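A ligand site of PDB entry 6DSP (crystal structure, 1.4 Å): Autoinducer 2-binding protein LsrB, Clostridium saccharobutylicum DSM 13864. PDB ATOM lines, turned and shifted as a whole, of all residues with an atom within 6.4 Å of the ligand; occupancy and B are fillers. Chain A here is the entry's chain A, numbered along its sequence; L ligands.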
ATOM      1  N   LYS A  29     -29.855   6.264 -30.542  1.00  0.00           N
ATOM      2  CA  LYS A  29     -29.766   7.069 -29.323  1.00  0.00           C
ATOM      3  C   LYS A  29     -29.215   8.455 -29.622  1.00  0.00           C
ATOM      4  O   LYS A  29     -29.611   9.433 -28.965  1.00  0.00           O
ATOM      5  CB  LYS A  29     -28.883   6.383 -28.276  1.00  0.00           C
ATOM      6  CG  LYS A  29     -29.485   5.180 -27.638  1.00  0.00           C
ATOM      7  CD  LYS A  29     -28.543   4.625 -26.542  1.00  0.00           C
ATOM      8  CE  LYS A  29     -29.056   3.360 -25.885  1.00  0.00           C
ATOM      9  NZ  LYS A  29     -27.991   2.848 -24.963  1.00  0.00           N
ATOM     10  N   ASN A  33     -22.259   9.006 -33.582  1.00  0.00           N
ATOM     11  CA  ASN A  33     -21.486   8.034 -32.829  1.00  0.00           C
ATOM     12  C   ASN A  33     -21.333   6.806 -33.714  1.00  0.00           C
ATOM     13  O   ASN A  33     -22.288   6.397 -34.398  1.00  0.00           O
ATOM     14  CB  ASN A  33     -22.286   7.684 -31.585  1.00  0.00           C
ATOM     15  CG  ASN A  33     -21.636   6.608 -30.725  1.00  0.00           C
ATOM     16  OD1 ASN A  33     -21.755   5.408 -30.983  1.00  0.00           O
ATOM     17  ND2 ASN A  33     -20.984   7.044 -29.650  1.00  0.00           N
ATOM     18  N   PHE A  35     -21.178   3.604 -33.402  1.00  0.00           N
ATOM     19  CA  PHE A  35     -22.074   2.457 -33.271  1.00  0.00           C
ATOM     20  C   PHE A  35     -23.336   2.671 -34.099  1.00  0.00           C
ATOM     21  O   PHE A  35     -23.790   1.761 -34.825  1.00  0.00           O
ATOM     22  CB  PHE A  35     -22.457   2.283 -31.800  1.00  0.00           C
ATOM     23  CG  PHE A  35     -23.422   1.154 -31.541  1.00  0.00           C
ATOM     24  CD1 PHE A  35     -22.999  -0.171 -31.412  1.00  0.00           C
ATOM     25  CD2 PHE A  35     -24.770   1.422 -31.505  1.00  0.00           C
ATOM     26  CE1 PHE A  35     -23.906  -1.204 -31.190  1.00  0.00           C
ATOM     27  CE2 PHE A  35     -25.703   0.410 -31.274  1.00  0.00           C
ATOM     28  CZ  PHE A  35     -25.258  -0.911 -31.136  1.00  0.00           C
ATOM     29  N   PHE A  36     -23.914   3.860 -33.996  1.00  0.00           N
ATOM     30  CA  PHE A  36     -25.182   4.150 -34.643  1.00  0.00           C
ATOM     31  C   PHE A  36     -24.999   4.400 -36.127  1.00  0.00           C
ATOM     32  O   PHE A  36     -25.835   3.986 -36.936  1.00  0.00           O
ATOM     33  CB  PHE A  36     -25.862   5.301 -33.919  1.00  0.00           C
ATOM     34  CG  PHE A  36     -26.261   4.895 -32.535  1.00  0.00           C
ATOM     35  CD1 PHE A  36     -27.342   4.039 -32.353  1.00  0.00           C
ATOM     36  CD2 PHE A  36     -25.527   5.246 -31.412  1.00  0.00           C
ATOM     37  CE1 PHE A  36     -27.683   3.539 -31.101  1.00  0.00           C
ATOM     38  CE2 PHE A  36     -25.900   4.751 -30.150  1.00  0.00           C
ATOM     39  CZ  PHE A  36     -26.996   3.913 -30.005  1.00  0.00           C
ATOM     40  N   SER A  85     -33.895   2.927 -30.752  1.00  0.00           N
ATOM     41  CA  SER A  85     -33.052   2.610 -29.593  1.00  0.00           C
ATOM     42  C   SER A  85     -33.186   3.763 -28.603  1.00  0.00           C
ATOM     43  O   SER A  85     -32.864   4.918 -28.932  1.00  0.00           O
ATOM     44  CB  SER A  85     -31.590   2.437 -29.979  1.00  0.00           C
ATOM     45  OG  SER A  85     -30.854   2.212 -28.786  1.00  0.00           O
ATOM     46  N   ASP A 110     -31.479  -2.489 -29.722  1.00  0.00           N
ATOM     47  CA  ASP A 110     -30.355  -1.999 -28.918  1.00  0.00           C
ATOM     48  C   ASP A 110     -30.737  -1.707 -27.471  1.00  0.00           C
ATOM     49  O   ASP A 110     -30.330  -2.446 -26.567  1.00  0.00           O
ATOM     50  CB  ASP A 110     -29.668  -0.814 -29.621  1.00  0.00           C
ATOM     51  CG  ASP A 110     -28.515  -0.249 -28.824  1.00  0.00           C
ATOM     52  OD1 ASP A 110     -27.674  -1.061 -28.357  1.00  0.00           O
ATOM     53  OD2 ASP A 110     -28.405   1.010 -28.735  1.00  0.00           O
ATOM     54  N   SER A 111     -31.565  -0.699 -27.222  1.00  0.00           N
ATOM     55  CA  SER A 111     -32.037  -0.382 -25.879  1.00  0.00           C
ATOM     56  C   SER A 111     -33.557  -0.255 -25.881  1.00  0.00           C
ATOM     57  O   SER A 111     -34.117   0.592 -26.586  1.00  0.00           O
ATOM     58  CB  SER A 111     -31.392   0.902 -25.341  1.00  0.00           C
ATOM     59  OG  SER A 111     -31.799   1.019 -23.987  1.00  0.00           O
ATOM     60  N   GLN A 124     -29.069  -7.364 -28.774  1.00  0.00           N
ATOM     61  CA  GLN A 124     -27.755  -7.937 -28.929  1.00  0.00           C
ATOM     62  C   GLN A 124     -27.453  -9.062 -27.932  1.00  0.00           C
ATOM     63  O   GLN A 124     -26.444  -9.755 -28.111  1.00  0.00           O
ATOM     64  CB  GLN A 124     -26.685  -6.840 -28.792  1.00  0.00           C
ATOM     65  CG  GLN A 124     -26.768  -5.980 -27.508  1.00  0.00           C
ATOM     66  CD  GLN A 124     -27.603  -4.712 -27.667  1.00  0.00           C
ATOM     67  OE1 GLN A 124     -28.711  -4.754 -28.221  1.00  0.00           O
ATOM     68  NE2 GLN A 124     -27.125  -3.608 -27.113  1.00  0.00           N
ATOM     69  N   VAL A 165     -30.965   4.512 -18.759  1.00  0.00           N
ATOM     70  CA  VAL A 165     -31.155   3.791 -20.012  1.00  0.00           C
ATOM     71  C   VAL A 165     -31.314   2.292 -19.755  1.00  0.00           C
ATOM     72  O   VAL A 165     -30.616   1.701 -18.924  1.00  0.00           O
ATOM     73  CB  VAL A 165     -29.977   4.124 -20.956  1.00  0.00           C
ATOM     74  CG1 VAL A 165     -28.642   3.615 -20.435  1.00  0.00           C
ATOM     75  CG2 VAL A 165     -30.269   3.605 -22.357  1.00  0.00           C
ATOM     76  N   ASP A 167     -30.685  -0.639 -21.630  1.00  0.00           N
ATOM     77  CA  ASP A 167     -29.710  -1.681 -21.933  1.00  0.00           C
ATOM     78  C   ASP A 167     -28.519  -1.662 -20.977  1.00  0.00           C
ATOM     79  O   ASP A 167     -28.222  -2.662 -20.299  1.00  0.00           O
ATOM     80  CB  ASP A 167     -29.281  -1.671 -23.421  1.00  0.00           C
ATOM     81  CG  ASP A 167     -28.540  -0.413 -23.880  1.00  0.00           C
ATOM     82  OD1 ASP A 167     -28.627   0.663 -23.247  1.00  0.00           O
ATOM     83  OD2 ASP A 167     -27.885  -0.545 -24.932  1.00  0.00           O
ATOM     84  N   GLN A 168     -27.849  -0.528 -20.878  1.00  0.00           N
ATOM     85  CA  GLN A 168     -26.578  -0.493 -20.175  1.00  0.00           C
ATOM     86  C   GLN A 168     -26.749  -0.705 -18.683  1.00  0.00           C
ATOM     87  O   GLN A 168     -25.888  -1.334 -18.053  1.00  0.00           O
ATOM     88  CB  GLN A 168     -25.864   0.810 -20.480  1.00  0.00           C
ATOM     89  CG  GLN A 168     -25.491   0.969 -21.927  1.00  0.00           C
ATOM     90  CD  GLN A 168     -24.878   2.295 -22.258  1.00  0.00           C
ATOM     91  OE1 GLN A 168     -24.546   3.114 -21.371  1.00  0.00           O
ATOM     92  NE2 GLN A 168     -24.714   2.528 -23.553  1.00  0.00           N
ATOM     93  N   TRP A 171     -27.058  -4.418 -17.908  1.00  0.00           N
ATOM     94  CA  TRP A 171     -25.774  -5.098 -17.894  1.00  0.00           C
ATOM     95  C   TRP A 171     -25.014  -4.823 -16.601  1.00  0.00           C
ATOM     96  O   TRP A 171     -24.360  -5.722 -16.087  1.00  0.00           O
ATOM     97  CB  TRP A 171     -24.935  -4.700 -19.100  1.00  0.00           C
ATOM     98  CG  TRP A 171     -25.651  -4.818 -20.411  1.00  0.00           C
ATOM     99  CD1 TRP A 171     -26.718  -5.586 -20.721  1.00  0.00           C
ATOM    100  CD2 TRP A 171     -25.366  -4.029 -21.578  1.00  0.00           C
ATOM    101  NE1 TRP A 171     -27.132  -5.340 -22.018  1.00  0.00           N
ATOM    102  CE2 TRP A 171     -26.309  -4.381 -22.556  1.00  0.00           C
ATOM    103  CE3 TRP A 171     -24.411  -3.049 -21.887  1.00  0.00           C
ATOM    104  CZ2 TRP A 171     -26.311  -3.796 -23.822  1.00  0.00           C
ATOM    105  CZ3 TRP A 171     -24.432  -2.465 -23.139  1.00  0.00           C
ATOM    106  CH2 TRP A 171     -25.386  -2.830 -24.093  1.00  0.00           C
ATOM    107  N   GLN A 198     -23.065  10.015 -23.321  1.00  0.00           N
ATOM    108  CA  GLN A 198     -22.791   9.780 -24.744  1.00  0.00           C
ATOM    109  C   GLN A 198     -22.235  11.011 -25.440  1.00  0.00           C
ATOM    110  O   GLN A 198     -22.345  11.144 -26.662  1.00  0.00           O
ATOM    111  CB  GLN A 198     -24.013   9.208 -25.484  1.00  0.00           C
ATOM    112  CG  GLN A 198     -24.452   7.911 -24.831  1.00  0.00           C
ATOM    113  CD  GLN A 198     -25.662   7.298 -25.452  1.00  0.00           C
ATOM    114  OE1 GLN A 198     -26.785   7.566 -25.024  1.00  0.00           O
ATOM    115  NE2 GLN A 198     -25.452   6.522 -26.491  1.00  0.00           N
ATOM    116  N   CYS A 222     -16.336  -0.063 -19.408  1.00  0.00           N
ATOM    117  CA  CYS A 222     -16.956   1.032 -20.171  1.00  0.00           C
ATOM    118  C   CYS A 222     -18.003   0.449 -21.121  1.00  0.00           C
ATOM    119  O   CYS A 222     -17.765   0.342 -22.326  1.00  0.00           O
ATOM    120  CB  CYS A 222     -15.867   1.752 -20.964  1.00  0.00           C
ATOM    121  SG  CYS A 222     -14.648   2.513 -19.854  1.00  0.00           S
ATOM    122  N   ASN A 223     -19.186   0.106 -20.570  1.00  0.00           N
ATOM    123  CA  ASN A 223     -20.255  -0.525 -21.332  1.00  0.00           C
ATOM    124  C   ASN A 223     -21.092   0.475 -22.129  1.00  0.00           C
ATOM    125  O   ASN A 223     -22.320   0.523 -22.020  1.00  0.00           O
ATOM    126  CB  ASN A 223     -21.163  -1.370 -20.414  1.00  0.00           C
ATOM    127  CG  ASN A 223     -21.628  -0.595 -19.165  1.00  0.00           C
ATOM    128  OD1 ASN A 223     -20.824   0.075 -18.496  1.00  0.00           O
ATOM    129  ND2 ASN A 223     -22.895  -0.743 -18.820  1.00  0.00           N
ATOM    130  N   ASP A 224     -20.405   1.281 -22.948  1.00  0.00           N
ATOM    131  CA  ASP A 224     -21.029   2.311 -23.762  1.00  0.00           C
ATOM    132  C   ASP A 224     -20.030   2.719 -24.844  1.00  0.00           C
ATOM    133  O   ASP A 224     -18.830   2.877 -24.581  1.00  0.00           O
ATOM    134  CB  ASP A 224     -21.411   3.522 -22.906  1.00  0.00           C
ATOM    135  CG  ASP A 224     -21.837   4.708 -23.770  1.00  0.00           C
ATOM    136  OD1 ASP A 224     -22.960   4.641 -24.329  1.00  0.00           O
ATOM    137  OD2 ASP A 224     -21.028   5.654 -23.935  1.00  0.00           O
ATOM    138  N   SER A 225     -20.539   2.919 -26.065  1.00  0.00           N
ATOM    139  CA  SER A 225     -19.722   3.165 -27.243  1.00  0.00           C
ATOM    140  C   SER A 225     -19.023   4.529 -27.255  1.00  0.00           C
ATOM    141  O   SER A 225     -18.151   4.755 -28.095  1.00  0.00           O
ATOM    142  CB  SER A 225     -20.506   2.979 -28.526  1.00  0.00           C
ATOM    143  OG  SER A 225     -21.479   3.990 -28.650  1.00  0.00           O
ATOM    144  N   THR A 226     -19.424   5.447 -26.366  1.00  0.00           N
ATOM    145  CA  THR A 226     -18.741   6.717 -26.182  1.00  0.00           C
ATOM    146  C   THR A 226     -17.794   6.651 -24.990  1.00  0.00           C
ATOM    147  O   THR A 226     -16.639   7.107 -25.074  1.00  0.00           O
ATOM    148  CB  THR A 226     -19.765   7.862 -25.941  1.00  0.00           C
ATOM    149  OG1 THR A 226     -20.772   7.834 -26.947  1.00  0.00           O
ATOM    150  CG2 THR A 226     -19.079   9.194 -26.041  1.00  0.00           C
ATOM    151  N   PHE A 250     -17.700  -1.888 -24.607  1.00  0.00           N
ATOM    152  CA  PHE A 250     -18.342  -2.148 -25.889  1.00  0.00           C
ATOM    153  C   PHE A 250     -18.165  -0.960 -26.839  1.00  0.00           C
ATOM    154  O   PHE A 250     -18.528   0.177 -26.480  1.00  0.00           O
ATOM    155  CB  PHE A 250     -19.841  -2.379 -25.699  1.00  0.00           C
ATOM    156  CG  PHE A 250     -20.204  -3.672 -25.001  1.00  0.00           C
ATOM    157  CD1 PHE A 250     -19.446  -4.864 -25.159  1.00  0.00           C
ATOM    158  CD2 PHE A 250     -21.352  -3.716 -24.214  1.00  0.00           C
ATOM    159  CE1 PHE A 250     -19.853  -6.044 -24.533  1.00  0.00           C
ATOM    160  CE2 PHE A 250     -21.772  -4.897 -23.598  1.00  0.00           C
ATOM    161  CZ  PHE A 250     -21.012  -6.065 -23.761  1.00  0.00           C
ATOM    162  N   ALA A 251     -17.706  -1.237 -28.062  1.00  0.00           N
ATOM    163  CA  ALA A 251     -17.675  -0.217 -29.105  1.00  0.00           C
ATOM    164  C   ALA A 251     -17.417  -0.913 -30.432  1.00  0.00           C
ATOM    165  O   ALA A 251     -16.814  -1.989 -30.471  1.00  0.00           O
ATOM    166  CB  ALA A 251     -16.596   0.852 -28.848  1.00  0.00           C
ATOM    167  N   SER A 252     -17.869  -0.292 -31.520  1.00  0.00           N
ATOM    168  CA  SER A 252     -17.577  -0.840 -32.834  1.00  0.00           C
ATOM    169  C   SER A 252     -16.060  -0.787 -33.079  1.00  0.00           C
ATOM    170  O   SER A 252     -15.362   0.117 -32.620  1.00  0.00           O
ATOM    171  CB  SER A 252     -18.400  -0.143 -33.928  1.00  0.00           C
ATOM    172  OG  SER A 252     -18.340   1.274 -33.845  1.00  0.00           O
ATOM    173  N   LEU A 270     -18.197  -6.285 -29.018  1.00  0.00           N
ATOM    174  CA  LEU A 270     -19.450  -5.774 -29.594  1.00  0.00           C
ATOM    175  C   LEU A 270     -20.162  -6.973 -30.207  1.00  0.00           C
ATOM    176  O   LEU A 270     -20.206  -8.048 -29.597  1.00  0.00           O
ATOM    177  CB  LEU A 270     -19.230  -4.632 -30.599  1.00  0.00           C
ATOM    178  CG  LEU A 270     -20.490  -3.746 -30.731  1.00  0.00           C
ATOM    179  CD1 LEU A 270     -20.682  -2.774 -29.565  1.00  0.00           C
ATOM    180  CD2 LEU A 270     -20.474  -3.002 -32.066  1.00  0.00           C
ATOM    181  N   TRP A 271     -20.744  -6.777 -31.383  1.00  0.00           N
ATOM    182  CA  TRP A 271     -21.636  -7.704 -32.068  1.00  0.00           C
ATOM    183  C   TRP A 271     -21.894  -7.023 -33.409  1.00  0.00           C
ATOM    184  O   TRP A 271     -21.441  -5.891 -33.639  1.00  0.00           O
ATOM    185  CB  TRP A 271     -22.950  -7.927 -31.264  1.00  0.00           C
ATOM    186  CG  TRP A 271     -23.602  -6.627 -30.867  1.00  0.00           C
ATOM    187  CD1 TRP A 271     -24.436  -5.860 -31.638  1.00  0.00           C
ATOM    188  CD2 TRP A 271     -23.435  -5.916 -29.630  1.00  0.00           C
ATOM    189  NE1 TRP A 271     -24.787  -4.708 -30.977  1.00  0.00           N
ATOM    190  CE2 TRP A 271     -24.191  -4.712 -29.731  1.00  0.00           C
ATOM    191  CE3 TRP A 271     -22.751  -6.184 -28.440  1.00  0.00           C
ATOM    192  CZ2 TRP A 271     -24.259  -3.790 -28.682  1.00  0.00           C
ATOM    193  CZ3 TRP A 271     -22.823  -5.254 -27.396  1.00  0.00           C
ATOM    194  CH2 TRP A 271     -23.575  -4.064 -27.538  1.00  0.00           C
ATOM    195  N   GLN A 276     -27.844  -6.019 -36.901  1.00  0.00           N
ATOM    196  CA  GLN A 276     -28.851  -5.745 -35.869  1.00  0.00           C
ATOM    197  C   GLN A 276     -29.799  -4.626 -36.300  1.00  0.00           C
ATOM    198  O   GLN A 276     -31.019  -4.765 -36.176  1.00  0.00           O
ATOM    199  CB  GLN A 276     -28.160  -5.373 -34.559  1.00  0.00           C
ATOM    200  CG  GLN A 276     -29.176  -5.194 -33.430  1.00  0.00           C
ATOM    201  CD  GLN A 276     -28.553  -4.663 -32.150  1.00  0.00           C
ATOM    202  OE1 GLN A 276     -27.403  -4.248 -32.141  1.00  0.00           O
ATOM    203  NE2 GLN A 276     -29.309  -4.728 -31.059  1.00  0.00           N
HETATM  204  O1  LIG L   1     -22.832  -0.228 -25.467  1.00  0.00           O
HETATM  205  C1  LIG L   1     -23.510   0.351 -26.603  1.00  0.00           C
HETATM  206  C2  LIG L   1     -22.831  -0.010 -27.947  1.00  0.00           C
HETATM  207  O2  LIG L   1     -23.207   1.853 -26.480  1.00  0.00           O
HETATM  208  C3  LIG L   1     -24.209   2.508 -27.124  1.00  0.00           C
HETATM  209  C4  LIG L   1     -25.286   1.481 -27.488  1.00  0.00           C
HETATM  210  O3  LIG L   1     -26.586   1.994 -27.189  1.00  0.00           O
HETATM  211  C5  LIG L   1     -24.870   0.280 -26.638  1.00  0.00           C
HETATM  212  O4  LIG L   1     -25.278  -0.922 -27.246  1.00  0.00           O
HETATM  213  O5  LIG L   1     -25.398   0.390 -25.338  1.00  0.00           O
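The side-chain carboxylate (OD1) of Asp 224 lies within hydrogen-bond range of the side-chain amide nitrogen (NE2) of Gln 168.
The side-chain hydroxyl (OG) of Ser 225 is in hydrogen-bond range of the side-chain amide oxygen (OD1) of Asn 33, 2.7 Å away.
OD1 of Asn 33 lies within hydrogen-bond range of N of Phe 35, at 3.1 Å.
The backbone NH (N) of Phe 250 lies within hydrogen-bond range of the backbone carbonyl oxygen (O) of Cys 222 (3.2 Å).
The side-chain hydroxyl of Ser 111 lies within hydrogen-bond range of the backbone NH of Asp 167, at 3.1 Å.
N of Ser 225 sits close to O of Phe 250.
N of Asp 110 lies close to NE2 of Gln 276.
OD2 of Asp 110 lies within hydrogen-bond range of OG of Ser 85 (2.7 Å).
An oxygen (O2) of the ligand sits at hydrogen-bond distance from the backbone NH (N) of Ser 225 (2.9 Å).
An oxygen (O4) of the ligand sits at hydrogen-bond distance from the side-chain amide nitrogen (NE2) of Gln 124 (3.3 Å).
NE2 of Gln 168 sits at hydrogen-bond distance from O5 of the ligand (2.9 Å).
OD2 of Asp 110 lies within hydrogen-bond range of O3 of the ligand (2.6 Å).
The side-chain carboxylate of Asp 167 sits at hydrogen-bond distance from an oxygen (O5) of the ligand (2.7 Å).
NZ of Lys 29 lies within hydrogen-bond range of O3 of the ligand (2.8 Å).
Phe 35 touches the ligand (CD1 to C2, 3.5 Å).
Phe 36 touches the ligand.
Trp 171 touches the ligand.
O of Asn 223 touches O1 of the ligand (3.6 Å).
CA of Asp 224 touches O2 of the ligand, at 3.5 Å.
CB of Phe 250 touches O1 of the ligand (3.7 Å).
Leu 270 touches the ligand (CD1 to C2, 3.9 Å).
CZ2 of Trp 271 touches O4 of the ligand (3.4 Å).
Of the 24 residues printed, 14 come within 4 Å of the ligand.
The nearest printed residue that does not touch the ligand is Gln 198 (4.2 Å).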
